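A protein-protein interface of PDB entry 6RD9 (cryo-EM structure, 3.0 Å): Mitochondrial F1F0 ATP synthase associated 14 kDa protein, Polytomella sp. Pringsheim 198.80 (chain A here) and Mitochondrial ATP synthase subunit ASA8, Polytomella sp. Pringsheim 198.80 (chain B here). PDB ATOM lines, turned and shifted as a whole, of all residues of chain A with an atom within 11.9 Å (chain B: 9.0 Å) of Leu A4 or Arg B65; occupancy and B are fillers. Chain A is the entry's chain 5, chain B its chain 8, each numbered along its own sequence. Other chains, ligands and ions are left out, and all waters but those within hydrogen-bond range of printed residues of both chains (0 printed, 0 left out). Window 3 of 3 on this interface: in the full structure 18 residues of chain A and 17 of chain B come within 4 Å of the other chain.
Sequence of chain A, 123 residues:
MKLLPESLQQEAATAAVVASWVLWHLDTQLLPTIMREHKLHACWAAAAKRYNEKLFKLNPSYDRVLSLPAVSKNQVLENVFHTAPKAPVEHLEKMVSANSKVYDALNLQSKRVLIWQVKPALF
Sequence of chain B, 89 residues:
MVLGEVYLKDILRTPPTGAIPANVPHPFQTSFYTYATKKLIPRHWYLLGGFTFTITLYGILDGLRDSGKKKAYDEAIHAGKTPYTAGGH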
ATOM      1  N   MET A   1     -31.112 -24.726 -25.913  1.00  0.00           N
ATOM      2  CA  MET A   1     -31.050 -23.711 -24.876  1.00  0.00           C
ATOM      3  C   MET A   1     -29.774 -23.851 -24.064  1.00  0.00           C
ATOM      4  O   MET A   1     -28.844 -24.551 -24.460  1.00  0.00           O
ATOM      5  CB  MET A   1     -32.280 -23.801 -23.970  1.00  0.00           C
ATOM      6  CG  MET A   1     -32.460 -25.155 -23.304  1.00  0.00           C
ATOM      7  SD  MET A   1     -34.165 -25.584 -22.918  1.00  0.00           S
ATOM      8  CE  MET A   1     -34.971 -25.203 -24.474  1.00  0.00           C
ATOM      9  N   LYS A   2     -29.735 -23.164 -22.928  1.00  0.00           N
ATOM     10  CA  LYS A   2     -28.599 -23.229 -22.016  1.00  0.00           C
ATOM     11  C   LYS A   2     -28.667 -24.538 -21.246  1.00  0.00           C
ATOM     12  O   LYS A   2     -29.538 -24.715 -20.393  1.00  0.00           O
ATOM     13  CB  LYS A   2     -28.620 -22.032 -21.068  1.00  0.00           C
ATOM     14  CG  LYS A   2     -27.544 -22.039 -20.012  1.00  0.00           C
ATOM     15  CD  LYS A   2     -26.191 -21.725 -20.608  1.00  0.00           C
ATOM     16  CE  LYS A   2     -25.156 -21.481 -19.527  1.00  0.00           C
ATOM     17  NZ  LYS A   2     -25.504 -20.329 -18.657  1.00  0.00           N
ATOM     18  N   LEU A   3     -27.776 -25.471 -21.565  1.00  0.00           N
ATOM     19  CA  LEU A   3     -27.643 -26.697 -20.797  1.00  0.00           C
ATOM     20  C   LEU A   3     -26.319 -26.763 -20.058  1.00  0.00           C
ATOM     21  O   LEU A   3     -26.308 -26.767 -18.828  1.00  0.00           O
ATOM     22  CB  LEU A   3     -27.794 -27.923 -21.689  1.00  0.00           C
ATOM     23  CG  LEU A   3     -29.127 -28.648 -21.671  1.00  0.00           C
ATOM     24  CD1 LEU A   3     -30.192 -27.868 -22.363  1.00  0.00           C
ATOM     25  CD2 LEU A   3     -28.915 -29.979 -22.335  1.00  0.00           C
ATOM     26  N   LEU A   4     -25.217 -26.782 -20.770  1.00  0.00           N
ATOM     27  CA  LEU A   4     -24.023 -26.811 -19.948  1.00  0.00           C
ATOM     28  C   LEU A   4     -23.562 -25.393 -19.667  1.00  0.00           C
ATOM     29  O   LEU A   4     -23.719 -24.515 -20.510  1.00  0.00           O
ATOM     30  CB  LEU A   4     -22.909 -27.588 -20.625  1.00  0.00           C
ATOM     31  CG  LEU A   4     -22.888 -29.063 -20.265  1.00  0.00           C
ATOM     32  CD1 LEU A   4     -23.860 -29.836 -21.097  1.00  0.00           C
ATOM     33  CD2 LEU A   4     -21.527 -29.625 -20.415  1.00  0.00           C
ATOM     34  N   PRO A   5     -23.041 -25.122 -18.489  1.00  0.00           N
ATOM     35  CA  PRO A   5     -22.540 -23.789 -18.190  1.00  0.00           C
ATOM     36  C   PRO A   5     -21.181 -23.570 -18.837  1.00  0.00           C
ATOM     37  O   PRO A   5     -20.614 -24.446 -19.475  1.00  0.00           O
ATOM     38  CB  PRO A   5     -22.456 -23.795 -16.674  1.00  0.00           C
ATOM     39  CG  PRO A   5     -22.269 -25.184 -16.326  1.00  0.00           C
ATOM     40  CD  PRO A   5     -23.026 -25.980 -17.299  1.00  0.00           C
ATOM     41  N   GLU A   6     -20.679 -22.354 -18.677  1.00  0.00           N
ATOM     42  CA  GLU A   6     -19.356 -22.029 -19.177  1.00  0.00           C
ATOM     43  C   GLU A   6     -18.277 -22.732 -18.371  1.00  0.00           C
ATOM     44  O   GLU A   6     -17.261 -23.156 -18.929  1.00  0.00           O
ATOM     45  CB  GLU A   6     -19.182 -20.516 -19.159  1.00  0.00           C
ATOM     46  CG  GLU A   6     -17.854 -20.012 -19.631  1.00  0.00           C
ATOM     47  CD  GLU A   6     -17.536 -18.661 -19.041  1.00  0.00           C
ATOM     48  OE1 GLU A   6     -16.362 -18.247 -19.099  1.00  0.00           O
ATOM     49  OE2 GLU A   6     -18.464 -18.011 -18.520  1.00  0.00           O
ATOM     50  N   SER A   7     -18.491 -22.893 -17.074  1.00  0.00           N
ATOM     51  CA  SER A   7     -17.633 -23.727 -16.248  1.00  0.00           C
ATOM     52  C   SER A   7     -18.525 -24.515 -15.313  1.00  0.00           C
ATOM     53  O   SER A   7     -19.371 -23.933 -14.640  1.00  0.00           O
ATOM     54  CB  SER A   7     -16.640 -22.896 -15.458  1.00  0.00           C
ATOM     55  OG  SER A   7     -15.615 -23.704 -14.927  1.00  0.00           O
ATOM     56  N   LEU A   8     -18.360 -25.832 -15.290  1.00  0.00           N
ATOM     57  CA  LEU A   8     -19.109 -26.639 -14.343  1.00  0.00           C
ATOM     58  C   LEU A   8     -18.521 -26.542 -12.954  1.00  0.00           C
ATOM     59  O   LEU A   8     -19.242 -26.692 -11.974  1.00  0.00           O
ATOM     60  CB  LEU A   8     -19.126 -28.093 -14.777  1.00  0.00           C
ATOM     61  CG  LEU A   8     -20.137 -28.552 -15.806  1.00  0.00           C
ATOM     62  CD1 LEU A   8     -19.644 -29.844 -16.355  1.00  0.00           C
ATOM     63  CD2 LEU A   8     -21.475 -28.732 -15.186  1.00  0.00           C
ATOM     64  N   GLN A   9     -17.214 -26.332 -12.849  1.00  0.00           N
ATOM     65  CA  GLN A   9     -16.588 -26.201 -11.548  1.00  0.00           C
ATOM     66  C   GLN A   9     -16.931 -24.877 -10.904  1.00  0.00           C
ATOM     67  O   GLN A   9     -16.959 -24.777  -9.682  1.00  0.00           O
ATOM     68  CB  GLN A   9     -15.084 -26.325 -11.685  1.00  0.00           C
ATOM     69  CG  GLN A   9     -14.357 -26.551 -10.418  1.00  0.00           C
ATOM     70  CD  GLN A   9     -12.902 -26.706 -10.652  1.00  0.00           C
ATOM     71  OE1 GLN A   9     -12.308 -25.933 -11.375  1.00  0.00           O
ATOM     72  NE2 GLN A   9     -12.313 -27.718 -10.058  1.00  0.00           N
ATOM     73  N   GLN A  10     -17.182 -23.848 -11.696  1.00  0.00           N
ATOM     74  CA  GLN A  10     -17.567 -22.573 -11.126  1.00  0.00           C
ATOM     75  C   GLN A  10     -18.986 -22.617 -10.596  1.00  0.00           C
ATOM     76  O   GLN A  10     -19.298 -21.959  -9.605  1.00  0.00           O
ATOM     77  CB  GLN A  10     -17.420 -21.488 -12.173  1.00  0.00           C
ATOM     78  CG  GLN A  10     -17.706 -20.116 -11.705  1.00  0.00           C
ATOM     79  CD  GLN A  10     -18.172 -19.251 -12.808  1.00  0.00           C
ATOM     80  OE1 GLN A  10     -18.662 -19.729 -13.816  1.00  0.00           O
ATOM     81  NE2 GLN A  10     -18.022 -17.965 -12.638  1.00  0.00           N
ATOM     82  N   GLU A  11     -19.865 -23.373 -11.243  1.00  0.00           N
ATOM     83  CA  GLU A  11     -21.205 -23.532 -10.707  1.00  0.00           C
ATOM     84  C   GLU A  11     -21.274 -24.530  -9.576  1.00  0.00           C
ATOM     85  O   GLU A  11     -22.138 -24.406  -8.714  1.00  0.00           O
ATOM     86  CB  GLU A  11     -22.177 -23.957 -11.786  1.00  0.00           C
ATOM     87  CG  GLU A  11     -22.701 -22.854 -12.628  1.00  0.00           C
ATOM     88  CD  GLU A  11     -23.866 -23.320 -13.469  1.00  0.00           C
ATOM     89  OE1 GLU A  11     -24.086 -24.537 -13.533  1.00  0.00           O
ATOM     90  OE2 GLU A  11     -24.590 -22.482 -14.036  1.00  0.00           O
ATOM     91  N   ALA A  12     -20.426 -25.541  -9.572  1.00  0.00           N
ATOM     92  CA  ALA A  12     -20.401 -26.448  -8.442  1.00  0.00           C
ATOM     93  C   ALA A  12     -19.801 -25.789  -7.225  1.00  0.00           C
ATOM     94  O   ALA A  12     -20.210 -26.091  -6.107  1.00  0.00           O
ATOM     95  CB  ALA A  12     -19.612 -27.702  -8.778  1.00  0.00           C
ATOM     96  N   TYR B  58     -15.935 -32.051 -10.869  1.00  0.00           N
ATOM     97  CA  TYR B  58     -16.411 -31.180 -11.925  1.00  0.00           C
ATOM     98  C   TYR B  58     -15.280 -30.411 -12.561  1.00  0.00           C
ATOM     99  O   TYR B  58     -15.476 -29.800 -13.605  1.00  0.00           O
ATOM    100  CB  TYR B  58     -17.449 -30.213 -11.391  1.00  0.00           C
ATOM    101  CG  TYR B  58     -18.845 -30.753 -11.325  1.00  0.00           C
ATOM    102  CD1 TYR B  58     -19.101 -32.027 -10.885  1.00  0.00           C
ATOM    103  CD2 TYR B  58     -19.904 -29.977 -11.691  1.00  0.00           C
ATOM    104  CE1 TYR B  58     -20.366 -32.504 -10.820  1.00  0.00           C
ATOM    105  CE2 TYR B  58     -21.167 -30.449 -11.626  1.00  0.00           C
ATOM    106  CZ  TYR B  58     -21.388 -31.705 -11.191  1.00  0.00           C
ATOM    107  OH  TYR B  58     -22.658 -32.170 -11.134  1.00  0.00           O
ATOM    108  N   GLY B  59     -14.106 -30.409 -11.941  1.00  0.00           N
ATOM    109  CA  GLY B  59     -12.907 -29.946 -12.600  1.00  0.00           C
ATOM    110  C   GLY B  59     -12.244 -30.988 -13.459  1.00  0.00           C
ATOM    111  O   GLY B  59     -11.463 -30.636 -14.342  1.00  0.00           O
ATOM    112  N   ILE B  60     -12.512 -32.265 -13.203  1.00  0.00           N
ATOM    113  CA  ILE B  60     -12.165 -33.301 -14.165  1.00  0.00           C
ATOM    114  C   ILE B  60     -13.026 -33.155 -15.406  1.00  0.00           C
ATOM    115  O   ILE B  60     -12.523 -33.165 -16.528  1.00  0.00           O
ATOM    116  CB  ILE B  60     -12.331 -34.699 -13.548  1.00  0.00           C
ATOM    117  CG1 ILE B  60     -11.544 -34.851 -12.253  1.00  0.00           C
ATOM    118  CG2 ILE B  60     -11.907 -35.747 -14.509  1.00  0.00           C
ATOM    119  CD1 ILE B  60     -10.134 -34.512 -12.350  1.00  0.00           C
ATOM    120  N   LEU B  61     -14.333 -32.988 -15.222  1.00  0.00           N
ATOM    121  CA  LEU B  61     -15.250 -32.897 -16.349  1.00  0.00           C
ATOM    122  C   LEU B  61     -15.107 -31.588 -17.102  1.00  0.00           C
ATOM    123  O   LEU B  61     -15.493 -31.506 -18.264  1.00  0.00           O
ATOM    124  CB  LEU B  61     -16.687 -33.045 -15.875  1.00  0.00           C
ATOM    125  CG  LEU B  61     -17.006 -34.270 -15.040  1.00  0.00           C
ATOM    126  CD1 LEU B  61     -18.459 -34.291 -14.683  1.00  0.00           C
ATOM    127  CD2 LEU B  61     -16.625 -35.510 -15.779  1.00  0.00           C
ATOM    128  N   ASP B  62     -14.604 -30.548 -16.459  1.00  0.00           N
ATOM    129  CA  ASP B  62     -14.273 -29.335 -17.182  1.00  0.00           C
ATOM    130  C   ASP B  62     -12.959 -29.487 -17.916  1.00  0.00           C
ATOM    131  O   ASP B  62     -12.724 -28.804 -18.914  1.00  0.00           O
ATOM    132  CB  ASP B  62     -14.186 -28.156 -16.224  1.00  0.00           C
ATOM    133  CG  ASP B  62     -15.461 -27.371 -16.149  1.00  0.00           C
ATOM    134  OD1 ASP B  62     -16.428 -27.737 -16.838  1.00  0.00           O
ATOM    135  OD2 ASP B  62     -15.485 -26.368 -15.413  1.00  0.00           O
ATOM    136  N   GLY B  63     -12.085 -30.355 -17.419  1.00  0.00           N
ATOM    137  CA  GLY B  63     -10.868 -30.668 -18.130  1.00  0.00           C
ATOM    138  C   GLY B  63     -11.092 -31.590 -19.297  1.00  0.00           C
ATOM    139  O   GLY B  63     -10.387 -31.490 -20.300  1.00  0.00           O
ATOM    140  N   LEU B  64     -12.059 -32.498 -19.193  1.00  0.00           N
ATOM    141  CA  LEU B  64     -12.389 -33.352 -20.325  1.00  0.00           C
ATOM    142  C   LEU B  64     -13.094 -32.575 -21.413  1.00  0.00           C
ATOM    143  O   LEU B  64     -12.994 -32.929 -22.587  1.00  0.00           O
ATOM    144  CB  LEU B  64     -13.273 -34.514 -19.897  1.00  0.00           C
ATOM    145  CG  LEU B  64     -12.776 -35.510 -18.865  1.00  0.00           C
ATOM    146  CD1 LEU B  64     -13.665 -36.709 -18.878  1.00  0.00           C
ATOM    147  CD2 LEU B  64     -11.359 -35.898 -19.105  1.00  0.00           C
ATOM    148  N   ARG B  65     -13.816 -31.531 -21.046  1.00  0.00           N
ATOM    149  CA  ARG B  65     -14.566 -30.768 -22.027  1.00  0.00           C
ATOM    150  C   ARG B  65     -13.667 -29.840 -22.824  1.00  0.00           C
ATOM    151  O   ARG B  65     -13.924 -29.598 -24.003  1.00  0.00           O
ATOM    152  CB  ARG B  65     -15.664 -29.982 -21.332  1.00  0.00           C
ATOM    153  CG  ARG B  65     -16.655 -29.369 -22.261  1.00  0.00           C
ATOM    154  CD  ARG B  65     -18.006 -29.355 -21.647  1.00  0.00           C
ATOM    155  NE  ARG B  65     -18.031 -28.529 -20.456  1.00  0.00           N
ATOM    156  CZ  ARG B  65     -18.534 -27.303 -20.421  1.00  0.00           C
ATOM    157  NH1 ARG B  65     -18.523 -26.615 -19.291  1.00  0.00           N
ATOM    158  NH2 ARG B  65     -19.053 -26.768 -21.516  1.00  0.00           N
ATOM    159  N   ASP B  66     -12.614 -29.303 -22.217  1.00  0.00           N
ATOM    160  CA  ASP B  66     -11.665 -28.495 -22.972  1.00  0.00           C
ATOM    161  C   ASP B  66     -10.610 -29.307 -23.691  1.00  0.00           C
ATOM    162  O   ASP B  66     -10.075 -28.833 -24.690  1.00  0.00           O
ATOM    163  CB  ASP B  66     -10.957 -27.476 -22.088  1.00  0.00           C
ATOM    164  CG  ASP B  66     -11.620 -26.118 -22.124  1.00  0.00           C
ATOM    165  OD1 ASP B  66     -12.842 -26.029 -22.354  1.00  0.00           O
ATOM    166  OD2 ASP B  66     -10.898 -25.122 -21.942  1.00  0.00           O
ATOM    167  N   SER B  67     -10.288 -30.505 -23.229  1.00  0.00           N
ATOM    168  CA  SER B  67      -9.432 -31.347 -24.042  1.00  0.00           C
ATOM    169  C   SER B  67     -10.190 -31.964 -25.202  1.00  0.00           C
ATOM    170  O   SER B  67      -9.565 -32.468 -26.133  1.00  0.00           O
ATOM    171  CB  SER B  67      -8.788 -32.440 -23.201  1.00  0.00           C
ATOM    172  OG  SER B  67      -9.748 -33.375 -22.773  1.00  0.00           O
ATOM    173  N   GLY B  68     -11.519 -31.957 -25.157  1.00  0.00           N
ATOM    174  CA  GLY B  68     -12.305 -32.311 -26.317  1.00  0.00           C
ATOM    175  C   GLY B  68     -12.605 -31.153 -27.233  1.00  0.00           C
ATOM    176  O   GLY B  68     -12.948 -31.371 -28.393  1.00  0.00           O
ATOM    177  N   LYS B  69     -12.530 -29.929 -26.727  1.00  0.00           N
ATOM    178  CA  LYS B  69     -12.612 -28.755 -27.582  1.00  0.00           C
ATOM    179  C   LYS B  69     -11.309 -28.537 -28.319  1.00  0.00           C
ATOM    180  O   LYS B  69     -11.308 -28.095 -29.465  1.00  0.00           O
ATOM    181  CB  LYS B  69     -12.925 -27.517 -26.755  1.00  0.00           C
ATOM    182  CG  LYS B  69     -14.365 -27.166 -26.604  1.00  0.00           C
ATOM    183  CD  LYS B  69     -14.449 -25.951 -25.739  1.00  0.00           C
ATOM    184  CE  LYS B  69     -15.835 -25.407 -25.664  1.00  0.00           C
ATOM    185  NZ  LYS B  69     -15.821 -24.177 -24.851  1.00  0.00           N
ATOM    186  N   LYS B  70     -10.194 -28.806 -27.651  1.00  0.00           N
ATOM    187  CA  LYS B  70      -8.887 -28.663 -28.268  1.00  0.00           C
ATOM    188  C   LYS B  70      -8.659 -29.728 -29.316  1.00  0.00           C
ATOM    189  O   LYS B  70      -7.988 -29.475 -30.317  1.00  0.00           O
ATOM    190  CB  LYS B  70      -7.818 -28.743 -27.190  1.00  0.00           C
ATOM    191  CG  LYS B  70      -6.428 -28.438 -27.624  1.00  0.00           C
ATOM    192  CD  LYS B  70      -5.489 -28.595 -26.454  1.00  0.00           C
ATOM    193  CE  LYS B  70      -4.051 -28.373 -26.866  1.00  0.00           C
ATOM    194  NZ  LYS B  70      -3.639 -29.319 -27.928  1.00  0.00           N
ATOM    195  N   LYS B  71      -9.216 -30.917 -29.112  1.00  0.00           N
ATOM    196  CA  LYS B  71      -9.094 -31.976 -30.103  1.00  0.00           C
ATOM    197  C   LYS B  71      -9.888 -31.648 -31.357  1.00  0.00           C
ATOM    198  O   LYS B  71      -9.402 -31.852 -32.469  1.00  0.00           O
ATOM    199  CB  LYS B  71      -9.530 -33.300 -29.488  1.00  0.00           C
ATOM    200  CG  LYS B  71     -10.129 -34.303 -30.437  1.00  0.00           C
ATOM    201  CD  LYS B  71     -10.297 -35.641 -29.757  1.00  0.00           C
ATOM    202  CE  LYS B  71     -11.242 -36.539 -30.521  1.00  0.00           C
ATOM    203  NZ  LYS B  71     -10.814 -36.742 -31.920  1.00  0.00           N
ATOM    204  N   ALA B  72     -11.080 -31.100 -31.212  1.00  0.00           N
ATOM    205  CA  ALA B  72     -11.852 -30.723 -32.383  1.00  0.00           C
ATOM    206  C   ALA B  72     -11.394 -29.416 -33.005  1.00  0.00           C
ATOM    207  O   ALA B  72     -11.771 -29.126 -34.139  1.00  0.00           O
ATOM    208  CB  ALA B  72     -13.332 -30.620 -32.032  1.00  0.00           C
ATOM    209  N   TYR B  73     -10.623 -28.607 -32.287  1.00  0.00           N
ATOM    210  CA  TYR B  73     -10.119 -27.360 -32.851  1.00  0.00           C
ATOM    211  C   TYR B  73      -8.900 -27.607 -33.711  1.00  0.00           C
ATOM    212  O   TYR B  73      -8.789 -27.053 -34.807  1.00  0.00           O
ATOM    213  CB  TYR B  73      -9.770 -26.384 -31.739  1.00  0.00           C
ATOM    214  CG  TYR B  73      -9.650 -24.946 -32.149  1.00  0.00           C
ATOM    215  CD1 TYR B  73     -10.758 -24.137 -32.209  1.00  0.00           C
ATOM    216  CD2 TYR B  73      -8.423 -24.390 -32.424  1.00  0.00           C
ATOM    217  CE1 TYR B  73     -10.655 -22.821 -32.556  1.00  0.00           C
ATOM    218  CE2 TYR B  73      -8.312 -23.075 -32.776  1.00  0.00           C
ATOM    219  CZ  TYR B  73      -9.435 -22.298 -32.839  1.00  0.00           C
ATOM    220  OH  TYR B  73      -9.337 -20.980 -33.190  1.00  0.00           O
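O of Pro A5 is in hydrogen-bond range of NH1 of Arg B65, at 3.0 Å. The side-chain hydroxyl (OG) of Ser A7 sits at hydrogen-bond distance from the side-chain carboxylate (OD2) of Asp B62. The backbone NH (N) of Leu A8 sits at hydrogen-bond distance from the side-chain carboxylate (OD2) of Asp B62 (2.9 Å). The backbone NH (N) of Gln A9 sits at hydrogen-bond distance from the side-chain carboxylate (OD2) of Asp B62 (3.1 Å).
NH1 of Arg B65 is in salt-bridge range of OD1 of Asp B62.
NE of Arg B65 touches CD2 of Leu A4, 3.7 Å away. Glu A6 touches Arg B65. Leu A8 touches Tyr B58. Gln A9 touches Tyr B58. Gly B59 touches Gln A9 (CA to NE2, 3.4 Å). CB of Ala A12 touches CD2 of Tyr B58, at 3.7 Å.
Leu A4 touches just one residue of chain B: Arg B65 (3.7 Å). Arg B65 touches three residues of chain A. Asp B62 touches three residues of chain A. No residue of chain A comes within 4 Å of Gly B63. No residue of chain A comes within 4 Å of Leu B64. Asp B66 touches none of the printed residues of chain A. No residue of chain A comes within 4 Å of Lys B69. Of the printed residues of chain B, Glu A6 touches Arg B65 (3.7 Å). Of the printed residues of chain B, Gln A9 touches Tyr B58, Gly B59 and Asp B62. Lys A2 touches none of the printed residues of chain B. The nearest printed residue of chain A that does not touch Gly B59 is Leu A8 (6.0 Å).
Of the 16 printed residues of chain B, 4 touch a printed residue of chain A. Hydrophobic or aromatic side chains of chain B that line the printed part of chain A: Tyr B58. Of the 12 printed residues of chain A, 7 touch a printed residue of chain B. Hydrophobic or aromatic side chains of chain A within 4 Å of the printed part of chain B: Leu A4, Leu A8 and Ala A12. Along chain A the printed residues that touch a printed residue of chain B span positions 4 to 12. Among the printed residues, 10 pairs touch across the chains.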
